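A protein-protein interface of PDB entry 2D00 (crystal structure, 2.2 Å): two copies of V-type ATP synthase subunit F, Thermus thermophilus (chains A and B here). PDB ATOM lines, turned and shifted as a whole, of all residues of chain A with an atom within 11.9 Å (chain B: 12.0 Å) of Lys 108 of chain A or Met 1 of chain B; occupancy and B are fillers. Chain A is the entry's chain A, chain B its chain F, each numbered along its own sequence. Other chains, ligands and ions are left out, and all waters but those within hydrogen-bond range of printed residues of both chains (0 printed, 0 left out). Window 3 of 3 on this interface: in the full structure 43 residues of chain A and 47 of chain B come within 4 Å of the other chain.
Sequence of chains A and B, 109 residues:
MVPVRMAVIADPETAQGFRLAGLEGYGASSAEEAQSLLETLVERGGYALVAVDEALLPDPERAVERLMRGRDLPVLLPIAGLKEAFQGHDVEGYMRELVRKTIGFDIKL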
ATOM      1  N   GLU A  92      18.161  -0.832   8.133  1.00  0.00           N
ATOM      2  CA  GLU A  92      18.355   0.379   7.284  1.00  0.00           C
ATOM      3  C   GLU A  92      17.381   0.378   6.083  1.00  0.00           C
ATOM      4  O   GLU A  92      16.905   1.446   5.622  1.00  0.00           O
ATOM      5  CB  GLU A  92      19.819   0.447   6.735  1.00  0.00           C
ATOM      6  CG  GLU A  92      20.082   1.729   5.855  1.00  0.00           C
ATOM      7  CD  GLU A  92      21.521   1.806   5.232  1.00  0.00           C
ATOM      8  OE1 GLU A  92      21.752   1.323   4.071  1.00  0.00           O
ATOM      9  OE2 GLU A  92      22.427   2.401   5.915  1.00  0.00           O
ATOM     10  N   GLY A  93      17.137  -0.839   5.609  1.00  0.00           N
ATOM     11  CA  GLY A  93      16.417  -1.145   4.361  1.00  0.00           C
ATOM     12  C   GLY A  93      14.963  -1.022   4.676  1.00  0.00           C
ATOM     13  O   GLY A  93      14.253  -0.346   3.953  1.00  0.00           O
ATOM     14  N   MET A  95      13.830   0.809   7.259  1.00  0.00           N
ATOM     15  CA  MET A  95      13.604   2.219   7.337  1.00  0.00           C
ATOM     16  C   MET A  95      13.548   2.958   5.974  1.00  0.00           C
ATOM     17  O   MET A  95      12.825   3.901   5.811  1.00  0.00           O
ATOM     18  CB  MET A  95      14.706   2.823   8.195  1.00  0.00           C
ATOM     19  CG  MET A  95      14.741   2.254   9.723  1.00  0.00           C
ATOM     20  SD  MET A  95      13.141   2.575  10.548  1.00  0.00           S
ATOM     21  CE  MET A  95      12.876   4.287  10.395  1.00  0.00           C
ATOM     22  N   ARG A  96      14.332   2.518   4.991  1.00  0.00           N
ATOM     23  CA  ARG A  96      14.270   3.124   3.640  1.00  0.00           C
ATOM     24  C   ARG A  96      12.930   2.986   2.992  1.00  0.00           C
ATOM     25  O   ARG A  96      12.418   3.928   2.360  1.00  0.00           O
ATOM     26  CB  ARG A  96      15.344   2.571   2.723  1.00  0.00           C
ATOM     27  CG  ARG A  96      15.671   3.532   1.571  1.00  0.00           C
ATOM     28  CD  ARG A  96      16.648   2.901   0.615  1.00  0.00           C
ATOM     29  NE  ARG A  96      17.840   2.404   1.325  1.00  0.00           N
ATOM     30  CZ  ARG A  96      18.213   1.116   1.452  1.00  0.00           C
ATOM     31  NH1 ARG A  96      17.504   0.103   0.931  1.00  0.00           N
ATOM     32  NH2 ARG A  96      19.333   0.828   2.113  1.00  0.00           N
ATOM     33  N   GLU A  97      12.370   1.803   3.206  1.00  0.00           N
ATOM     34  CA  GLU A  97      11.118   1.411   2.636  1.00  0.00           C
ATOM     35  C   GLU A  97       9.989   2.024   3.417  1.00  0.00           C
ATOM     36  O   GLU A  97       8.988   2.497   2.894  1.00  0.00           O
ATOM     37  CB  GLU A  97      11.035  -0.110   2.602  1.00  0.00           C
ATOM     38  CG  GLU A  97      11.941  -0.745   1.562  1.00  0.00           C
ATOM     39  CD  GLU A  97      11.551  -0.416   0.124  1.00  0.00           C
ATOM     40  OE1 GLU A  97      10.701   0.476  -0.134  1.00  0.00           O
ATOM     41  OE2 GLU A  97      12.088  -1.112  -0.779  1.00  0.00           O
ATOM     42  N   LEU A  98      10.170   2.105   4.682  1.00  0.00           N
ATOM     43  CA  LEU A  98       9.258   2.898   5.439  1.00  0.00           C
ATOM     44  C   LEU A  98       9.136   4.352   4.982  1.00  0.00           C
ATOM     45  O   LEU A  98       8.045   4.888   4.799  1.00  0.00           O
ATOM     46  CB  LEU A  98       9.665   2.869   6.864  1.00  0.00           C
ATOM     47  CG  LEU A  98       8.639   3.438   7.798  1.00  0.00           C
ATOM     48  CD1 LEU A  98       7.256   2.925   7.526  1.00  0.00           C
ATOM     49  CD2 LEU A  98       9.115   3.138   9.277  1.00  0.00           C
ATOM     50  N   VAL A  99      10.232   5.037   4.827  1.00  0.00           N
ATOM     51  CA  VAL A  99      10.092   6.452   4.546  1.00  0.00           C
ATOM     52  C   VAL A  99       9.431   6.629   3.205  1.00  0.00           C
ATOM     53  O   VAL A  99       8.589   7.542   2.988  1.00  0.00           O
ATOM     54  CB  VAL A  99      11.454   7.084   4.450  1.00  0.00           C
ATOM     55  CG1 VAL A  99      11.401   8.412   3.693  1.00  0.00           C
ATOM     56  CG2 VAL A  99      12.023   7.246   5.833  1.00  0.00           C
ATOM     57  N   ARG A 100       9.871   5.772   2.277  1.00  0.00           N
ATOM     58  CA  ARG A 100       9.349   5.800   0.938  1.00  0.00           C
ATOM     59  C   ARG A 100       7.888   5.429   0.968  1.00  0.00           C
ATOM     60  O   ARG A 100       7.120   6.004   0.202  1.00  0.00           O
ATOM     61  CB  ARG A 100      10.129   4.881  -0.005  1.00  0.00           C
ATOM     62  CG  ARG A 100       9.723   5.008  -1.451  1.00  0.00           C
ATOM     63  CD  ARG A 100       9.783   3.637  -2.225  1.00  0.00           C
ATOM     64  NE  ARG A 100       9.031   2.540  -1.587  1.00  0.00           N
ATOM     65  CZ  ARG A 100       7.769   2.218  -1.862  1.00  0.00           C
ATOM     66  NH1 ARG A 100       7.078   2.878  -2.784  1.00  0.00           N
ATOM     67  NH2 ARG A 100       7.182   1.232  -1.198  1.00  0.00           N
ATOM     68  N   ILE A 103       6.312   8.970   2.459  1.00  0.00           N
ATOM     69  CA  ILE A 103       6.451  10.246   1.774  1.00  0.00           C
ATOM     70  C   ILE A 103       6.904  10.181   0.292  1.00  0.00           C
ATOM     71  O   ILE A 103       7.027  11.200  -0.375  1.00  0.00           O
ATOM     72  CB  ILE A 103       7.328  11.172   2.589  1.00  0.00           C
ATOM     73  CG1 ILE A 103       8.833  10.925   2.314  1.00  0.00           C
ATOM     74  CG2 ILE A 103       6.999  10.998   4.150  1.00  0.00           C
ATOM     75  CD1 ILE A 103       9.687  11.733   3.175  1.00  0.00           C
ATOM     76  N   GLY A 104       7.125   8.994  -0.231  1.00  0.00           N
ATOM     77  CA  GLY A 104       7.467   8.889  -1.634  1.00  0.00           C
ATOM     78  C   GLY A 104       8.946   8.924  -1.893  1.00  0.00           C
ATOM     79  O   GLY A 104       9.387   8.502  -2.925  1.00  0.00           O
ATOM     80  N   PHE A 105       9.740   9.371  -0.941  1.00  0.00           N
ATOM     81  CA  PHE A 105      11.160   9.617  -1.205  1.00  0.00           C
ATOM     82  C   PHE A 105      12.096   8.452  -0.894  1.00  0.00           C
ATOM     83  O   PHE A 105      12.210   8.025   0.280  1.00  0.00           O
ATOM     84  CB  PHE A 105      11.633  10.875  -0.415  1.00  0.00           C
ATOM     85  CG  PHE A 105      11.461  12.152  -1.191  1.00  0.00           C
ATOM     86  CD1 PHE A 105      10.251  12.819  -1.171  1.00  0.00           C
ATOM     87  CD2 PHE A 105      12.500  12.641  -1.981  1.00  0.00           C
ATOM     88  CE1 PHE A 105      10.089  13.981  -1.922  1.00  0.00           C
ATOM     89  CE2 PHE A 105      12.347  13.792  -2.726  1.00  0.00           C
ATOM     90  CZ  PHE A 105      11.141  14.459  -2.715  1.00  0.00           C
ATOM     91  N   ASP A 106      12.822   8.011  -1.910  1.00  0.00           N
ATOM     92  CA  ASP A 106      13.938   7.108  -1.715  1.00  0.00           C
ATOM     93  C   ASP A 106      15.134   7.889  -1.171  1.00  0.00           C
ATOM     94  O   ASP A 106      15.743   8.740  -1.857  1.00  0.00           O
ATOM     95  CB  ASP A 106      14.243   6.338  -3.011  1.00  0.00           C
ATOM     96  CG  ASP A 106      13.396   5.074  -3.122  1.00  0.00           C
ATOM     97  OD1 ASP A 106      13.272   4.373  -2.071  1.00  0.00           O
ATOM     98  OD2 ASP A 106      12.832   4.808  -4.207  1.00  0.00           O
ATOM     99  N   ILE A 107      15.412   7.652   0.123  1.00  0.00           N
ATOM    100  CA  ILE A 107      16.408   8.408   0.829  1.00  0.00           C
ATOM    101  C   ILE A 107      17.781   7.672   0.713  1.00  0.00           C
ATOM    102  O   ILE A 107      17.869   6.432   0.696  1.00  0.00           O
ATOM    103  CB  ILE A 107      15.892   8.836   2.254  1.00  0.00           C
ATOM    104  CG1 ILE A 107      17.030   9.352   3.120  1.00  0.00           C
ATOM    105  CG2 ILE A 107      15.233   7.665   3.035  1.00  0.00           C
ATOM    106  CD1 ILE A 107      16.578  10.154   4.335  1.00  0.00           C
ATOM    107  N   LYS A 108      18.816   8.493   0.539  1.00  0.00           N
ATOM    108  CA  LYS A 108      20.218   8.105   0.357  1.00  0.00           C
ATOM    109  C   LYS A 108      21.040   7.889   1.664  1.00  0.00           C
ATOM    110  O   LYS A 108      22.019   8.627   1.909  1.00  0.00           O
ATOM    111  CB  LYS A 108      20.915   9.226  -0.455  1.00  0.00           C
ATOM    112  CG  LYS A 108      20.807   9.141  -1.957  1.00  0.00           C
ATOM    113  CD  LYS A 108      19.370   9.211  -2.508  1.00  0.00           C
ATOM    114  CE  LYS A 108      19.384   8.881  -4.015  1.00  0.00           C
ATOM    115  NZ  LYS A 108      18.213   8.071  -4.413  1.00  0.00           N
ATOM    116  N   LEU A 109      20.674   6.902   2.491  1.00  0.00           N
ATOM    117  CA  LEU A 109      21.452   6.561   3.699  1.00  0.00           C
ATOM    118  C   LEU A 109      22.346   5.376   3.401  1.00  0.00           C
ATOM    119  O   LEU A 109      21.791   4.385   2.916  1.00  0.00           O
ATOM    120  CB  LEU A 109      20.531   6.162   4.845  1.00  0.00           C
ATOM    121  CG  LEU A 109      19.463   7.210   5.237  1.00  0.00           C
ATOM    122  CD1 LEU A 109      18.108   6.484   5.501  1.00  0.00           C
ATOM    123  CD2 LEU A 109      19.942   8.105   6.367  1.00  0.00           C
ATOM    124  OXT LEU A 109      23.575   5.326   3.621  1.00  0.00           O
ATOM    125  N   MET B   1      27.269  14.578  -4.766  1.00  0.00           N
ATOM    126  CA  MET B   1      25.959  14.332  -4.081  1.00  0.00           C
ATOM    127  C   MET B   1      26.168  13.731  -2.675  1.00  0.00           C
ATOM    128  O   MET B   1      26.704  12.610  -2.514  1.00  0.00           O
ATOM    129  CB  MET B   1      25.121  13.404  -4.948  1.00  0.00           C
ATOM    130  CG  MET B   1      23.774  13.041  -4.406  1.00  0.00           C
ATOM    131  SD  MET B   1      23.321  11.350  -4.902  1.00  0.00           S
ATOM    132  CE  MET B   1      23.825  10.396  -3.392  1.00  0.00           C
ATOM    133  N   VAL B   2      25.650  14.495  -1.648  1.00  0.00           N
ATOM    134  CA  VAL B   2      26.029  14.393  -0.246  1.00  0.00           C
ATOM    135  C   VAL B   2      25.157  13.290   0.510  1.00  0.00           C
ATOM    136  O   VAL B   2      24.004  12.906   0.041  1.00  0.00           O
ATOM    137  CB  VAL B   2      25.830  15.819   0.435  1.00  0.00           C
ATOM    138  CG1 VAL B   2      26.140  15.798   1.961  1.00  0.00           C
ATOM    139  CG2 VAL B   2      26.670  16.959  -0.381  1.00  0.00           C
ATOM    140  N   PRO B   3      25.712  12.682   1.580  1.00  0.00           N
ATOM    141  CA  PRO B   3      24.968  11.699   2.408  1.00  0.00           C
ATOM    142  C   PRO B   3      23.794  12.271   3.199  1.00  0.00           C
ATOM    143  O   PRO B   3      23.891  13.433   3.753  1.00  0.00           O
ATOM    144  CB  PRO B   3      26.033  11.160   3.372  1.00  0.00           C
ATOM    145  CG  PRO B   3      27.264  11.311   2.641  1.00  0.00           C
ATOM    146  CD  PRO B   3      27.119  12.705   1.998  1.00  0.00           C
ATOM    147  N   VAL B   4      22.673  11.494   3.165  1.00  0.00           N
ATOM    148  CA  VAL B   4      21.426  12.012   3.690  1.00  0.00           C
ATOM    149  C   VAL B   4      21.342  11.631   5.163  1.00  0.00           C
ATOM    150  O   VAL B   4      21.447  10.466   5.525  1.00  0.00           O
ATOM    151  CB  VAL B   4      20.238  11.437   2.982  1.00  0.00           C
ATOM    152  CG1 VAL B   4      19.025  11.738   3.732  1.00  0.00           C
ATOM    153  CG2 VAL B   4      20.152  11.967   1.566  1.00  0.00           C
ATOM    154  N   ARG B   5      21.122  12.617   6.007  1.00  0.00           N
ATOM    155  CA  ARG B   5      21.247  12.409   7.407  1.00  0.00           C
ATOM    156  C   ARG B   5      19.865  12.297   8.032  1.00  0.00           C
ATOM    157  O   ARG B   5      19.095  13.140   7.861  1.00  0.00           O
ATOM    158  CB  ARG B   5      22.008  13.608   7.912  1.00  0.00           C
ATOM    159  CG  ARG B   5      22.825  13.308   9.114  1.00  0.00           C
ATOM    160  CD  ARG B   5      24.385  13.099   8.756  1.00  0.00           C
ATOM    161  NE  ARG B   5      24.766  12.689  10.089  1.00  0.00           N
ATOM    162  CZ  ARG B   5      25.079  13.512  11.087  1.00  0.00           C
ATOM    163  NH1 ARG B   5      25.330  14.835  10.878  1.00  0.00           N
ATOM    164  NH2 ARG B   5      25.224  12.959  12.301  1.00  0.00           N
ATOM    165  N   MET B   6      19.560  11.217   8.696  1.00  0.00           N
ATOM    166  CA  MET B   6      18.326  10.956   9.327  1.00  0.00           C
ATOM    167  C   MET B   6      18.540  10.601  10.769  1.00  0.00           C
ATOM    168  O   MET B   6      19.402   9.781  11.115  1.00  0.00           O
ATOM    169  CB  MET B   6      17.612   9.756   8.651  1.00  0.00           C
ATOM    170  CG  MET B   6      16.374   9.216   9.374  1.00  0.00           C
ATOM    171  SD  MET B   6      15.647   7.737   8.574  1.00  0.00           S
ATOM    172  CE  MET B   6      16.524   6.416   9.424  1.00  0.00           C
ATOM    173  N   ALA B   7      17.682  11.112  11.627  1.00  0.00           N
ATOM    174  CA  ALA B   7      17.675  10.607  13.016  1.00  0.00           C
ATOM    175  C   ALA B   7      16.343   9.940  13.356  1.00  0.00           C
ATOM    176  O   ALA B   7      15.305  10.213  12.713  1.00  0.00           O
ATOM    177  CB  ALA B   7      17.885  11.815  13.923  1.00  0.00           C
ATOM    178  N   GLY B  22      23.677   0.755  13.218  1.00  0.00           N
ATOM    179  CA  GLY B  22      24.415   1.726  12.437  1.00  0.00           C
ATOM    180  C   GLY B  22      23.508   2.943  12.096  1.00  0.00           C
ATOM    181  O   GLY B  22      23.820   3.716  11.257  1.00  0.00           O
ATOM    182  N   LEU B  23      22.371   3.113  12.747  1.00  0.00           N
ATOM    183  CA  LEU B  23      21.533   4.272  12.537  1.00  0.00           C
ATOM    184  C   LEU B  23      21.625   5.272  13.708  1.00  0.00           C
ATOM    185  O   LEU B  23      22.057   4.934  14.855  1.00  0.00           O
ATOM    186  CB  LEU B  23      20.087   3.837  12.340  1.00  0.00           C
ATOM    187  CG  LEU B  23      19.687   2.883  11.226  1.00  0.00           C
ATOM    188  CD1 LEU B  23      18.230   3.081  10.850  1.00  0.00           C
ATOM    189  CD2 LEU B  23      20.480   3.113  10.020  1.00  0.00           C
ATOM    190  N   GLU B  24      21.183   6.491  13.468  1.00  0.00           N
ATOM    191  CA  GLU B  24      21.376   7.549  14.409  1.00  0.00           C
ATOM    192  C   GLU B  24      20.153   7.640  15.314  1.00  0.00           C
ATOM    193  O   GLU B  24      19.266   8.468  15.093  1.00  0.00           O
ATOM    194  CB  GLU B  24      21.763   8.861  13.648  1.00  0.00           C
ATOM    195  CG  GLU B  24      21.963  10.029  14.562  1.00  0.00           C
ATOM    196  CD  GLU B  24      22.741  11.307  13.921  1.00  0.00           C
ATOM    197  OE1 GLU B  24      22.467  12.452  14.406  1.00  0.00           O
ATOM    198  OE2 GLU B  24      23.606  11.092  13.022  1.00  0.00           O
ATOM    199  N   GLY B  46      22.073  19.497  10.351  1.00  0.00           N
ATOM    200  CA  GLY B  46      22.271  18.666   9.052  1.00  0.00           C
ATOM    201  C   GLY B  46      21.058  17.876   8.326  1.00  0.00           C
ATOM    202  O   GLY B  46      20.905  17.845   7.039  1.00  0.00           O
ATOM    203  N   TYR B  47      20.197  17.403   9.195  1.00  0.00           N
ATOM    204  CA  TYR B  47      19.241  16.255   9.105  1.00  0.00           C
ATOM    205  C   TYR B  47      18.221  16.517   8.085  1.00  0.00           C
ATOM    206  O   TYR B  47      17.680  17.632   8.047  1.00  0.00           O
ATOM    207  CB  TYR B  47      18.586  16.202  10.457  1.00  0.00           C
ATOM    208  CG  TYR B  47      19.630  15.766  11.477  1.00  0.00           C
ATOM    209  CD1 TYR B  47      19.904  14.445  11.700  1.00  0.00           C
ATOM    210  CD2 TYR B  47      20.456  16.701  12.062  1.00  0.00           C
ATOM    211  CE1 TYR B  47      20.858  14.050  12.594  1.00  0.00           C
ATOM    212  CE2 TYR B  47      21.415  16.332  12.927  1.00  0.00           C
ATOM    213  CZ  TYR B  47      21.573  14.988  13.219  1.00  0.00           C
ATOM    214  OH  TYR B  47      22.606  14.727  14.069  1.00  0.00           O
ATOM    215  N   ALA B  48      18.050  15.618   7.134  1.00  0.00           N
ATOM    216  CA  ALA B  48      17.023  15.826   6.150  1.00  0.00           C
ATOM    217  C   ALA B  48      15.625  15.382   6.773  1.00  0.00           C
ATOM    218  O   ALA B  48      14.533  15.870   6.354  1.00  0.00           O
ATOM    219  CB  ALA B  48      17.299  15.057   4.934  1.00  0.00           C
ATOM    220  N   LEU B  49      15.756  14.540   7.744  1.00  0.00           N
ATOM    221  CA  LEU B  49      14.642  13.766   8.275  1.00  0.00           C
ATOM    222  C   LEU B  49      14.805  13.272   9.729  1.00  0.00           C
ATOM    223  O   LEU B  49      15.858  12.855  10.149  1.00  0.00           O
ATOM    224  CB  LEU B  49      14.264  12.594   7.341  1.00  0.00           C
ATOM    225  CG  LEU B  49      13.148  11.559   7.701  1.00  0.00           C
ATOM    226  CD1 LEU B  49      11.799  12.148   7.380  1.00  0.00           C
ATOM    227  CD2 LEU B  49      13.323  10.475   6.815  1.00  0.00           C
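The backbone NH (N) of Val 4 of chain B is in hydrogen-bond range of the backbone carbonyl oxygen (O) of Lys 108 of chain A (3.2 Å).
Met 95 of chain A touches Leu 23 of chain B.
CG2 of Val 99 of chain A touches CD2 of Leu 49 of chain B, 3.6 Å away.
Ile 107 of chain A touches Val 4 of chain B (CD1 to CG1, 3.0 Å).
Met 1 of chain B touches Lys 108 of chain A (CE to CG, 3.6 Å).
Leu 109 of chain A touches Val 4 of chain B (CD2 to O, 2.9 Å).
CB of Met 6 of chain B touches CD2 of Leu 109 of chain A (3.7 Å).
No position is printed for both chains.
The backbone NH of Ala 7 of chain B is in hydrogen-bond range of the backbone carbonyl oxygen of Leu 49 of chain B (2.9 Å).
Of the printed residues of chain B, Met 95 of chain A touches Leu 23 (3.8 Å).
Arg 96 of chain A touches none of the printed residues of chain B.
Printed residues of chain B within 4 Å of Val 99 of chain A: Leu 49 (3.6 Å).
No residue of chain B comes within 4 Å of Asp 106 of chain A.
Of chain B, only Met 1 and Val 4 come within 4 Å of Lys 108 of chain A.
Of chain B, only Val 4 and Met 6 come within 4 Å of Leu 109 of chain A.
Met 1 of chain B touches just one residue of chain A: Lys 108 (3.6 Å).
No residue of chain A comes within 4 Å of Val 2 of chain B.
No residue of chain A comes within 4 Å of Pro 3 of chain B.
Of the printed residues of chain A, Val 4 of chain B touches Ile 107 (3.0 Å), Lys 108 (3.2 Å) and Leu 109 (2.9 Å).
Of the printed residues of chain A, Met 6 of chain B touches Leu 109 (3.7 Å).
Printed residues of chain A within 4 Å of Leu 23 of chain B: Met 95 (3.8 Å).
The nearest residue of chain A that does not touch Met 1 of chain B is Leu 109 of chain A (7.5 Å).
Of the 15 printed residues of chain A, 5 touch a printed residue of chain B.
Of the 14 printed residues of chain B, 5 touch a printed residue of chain A.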
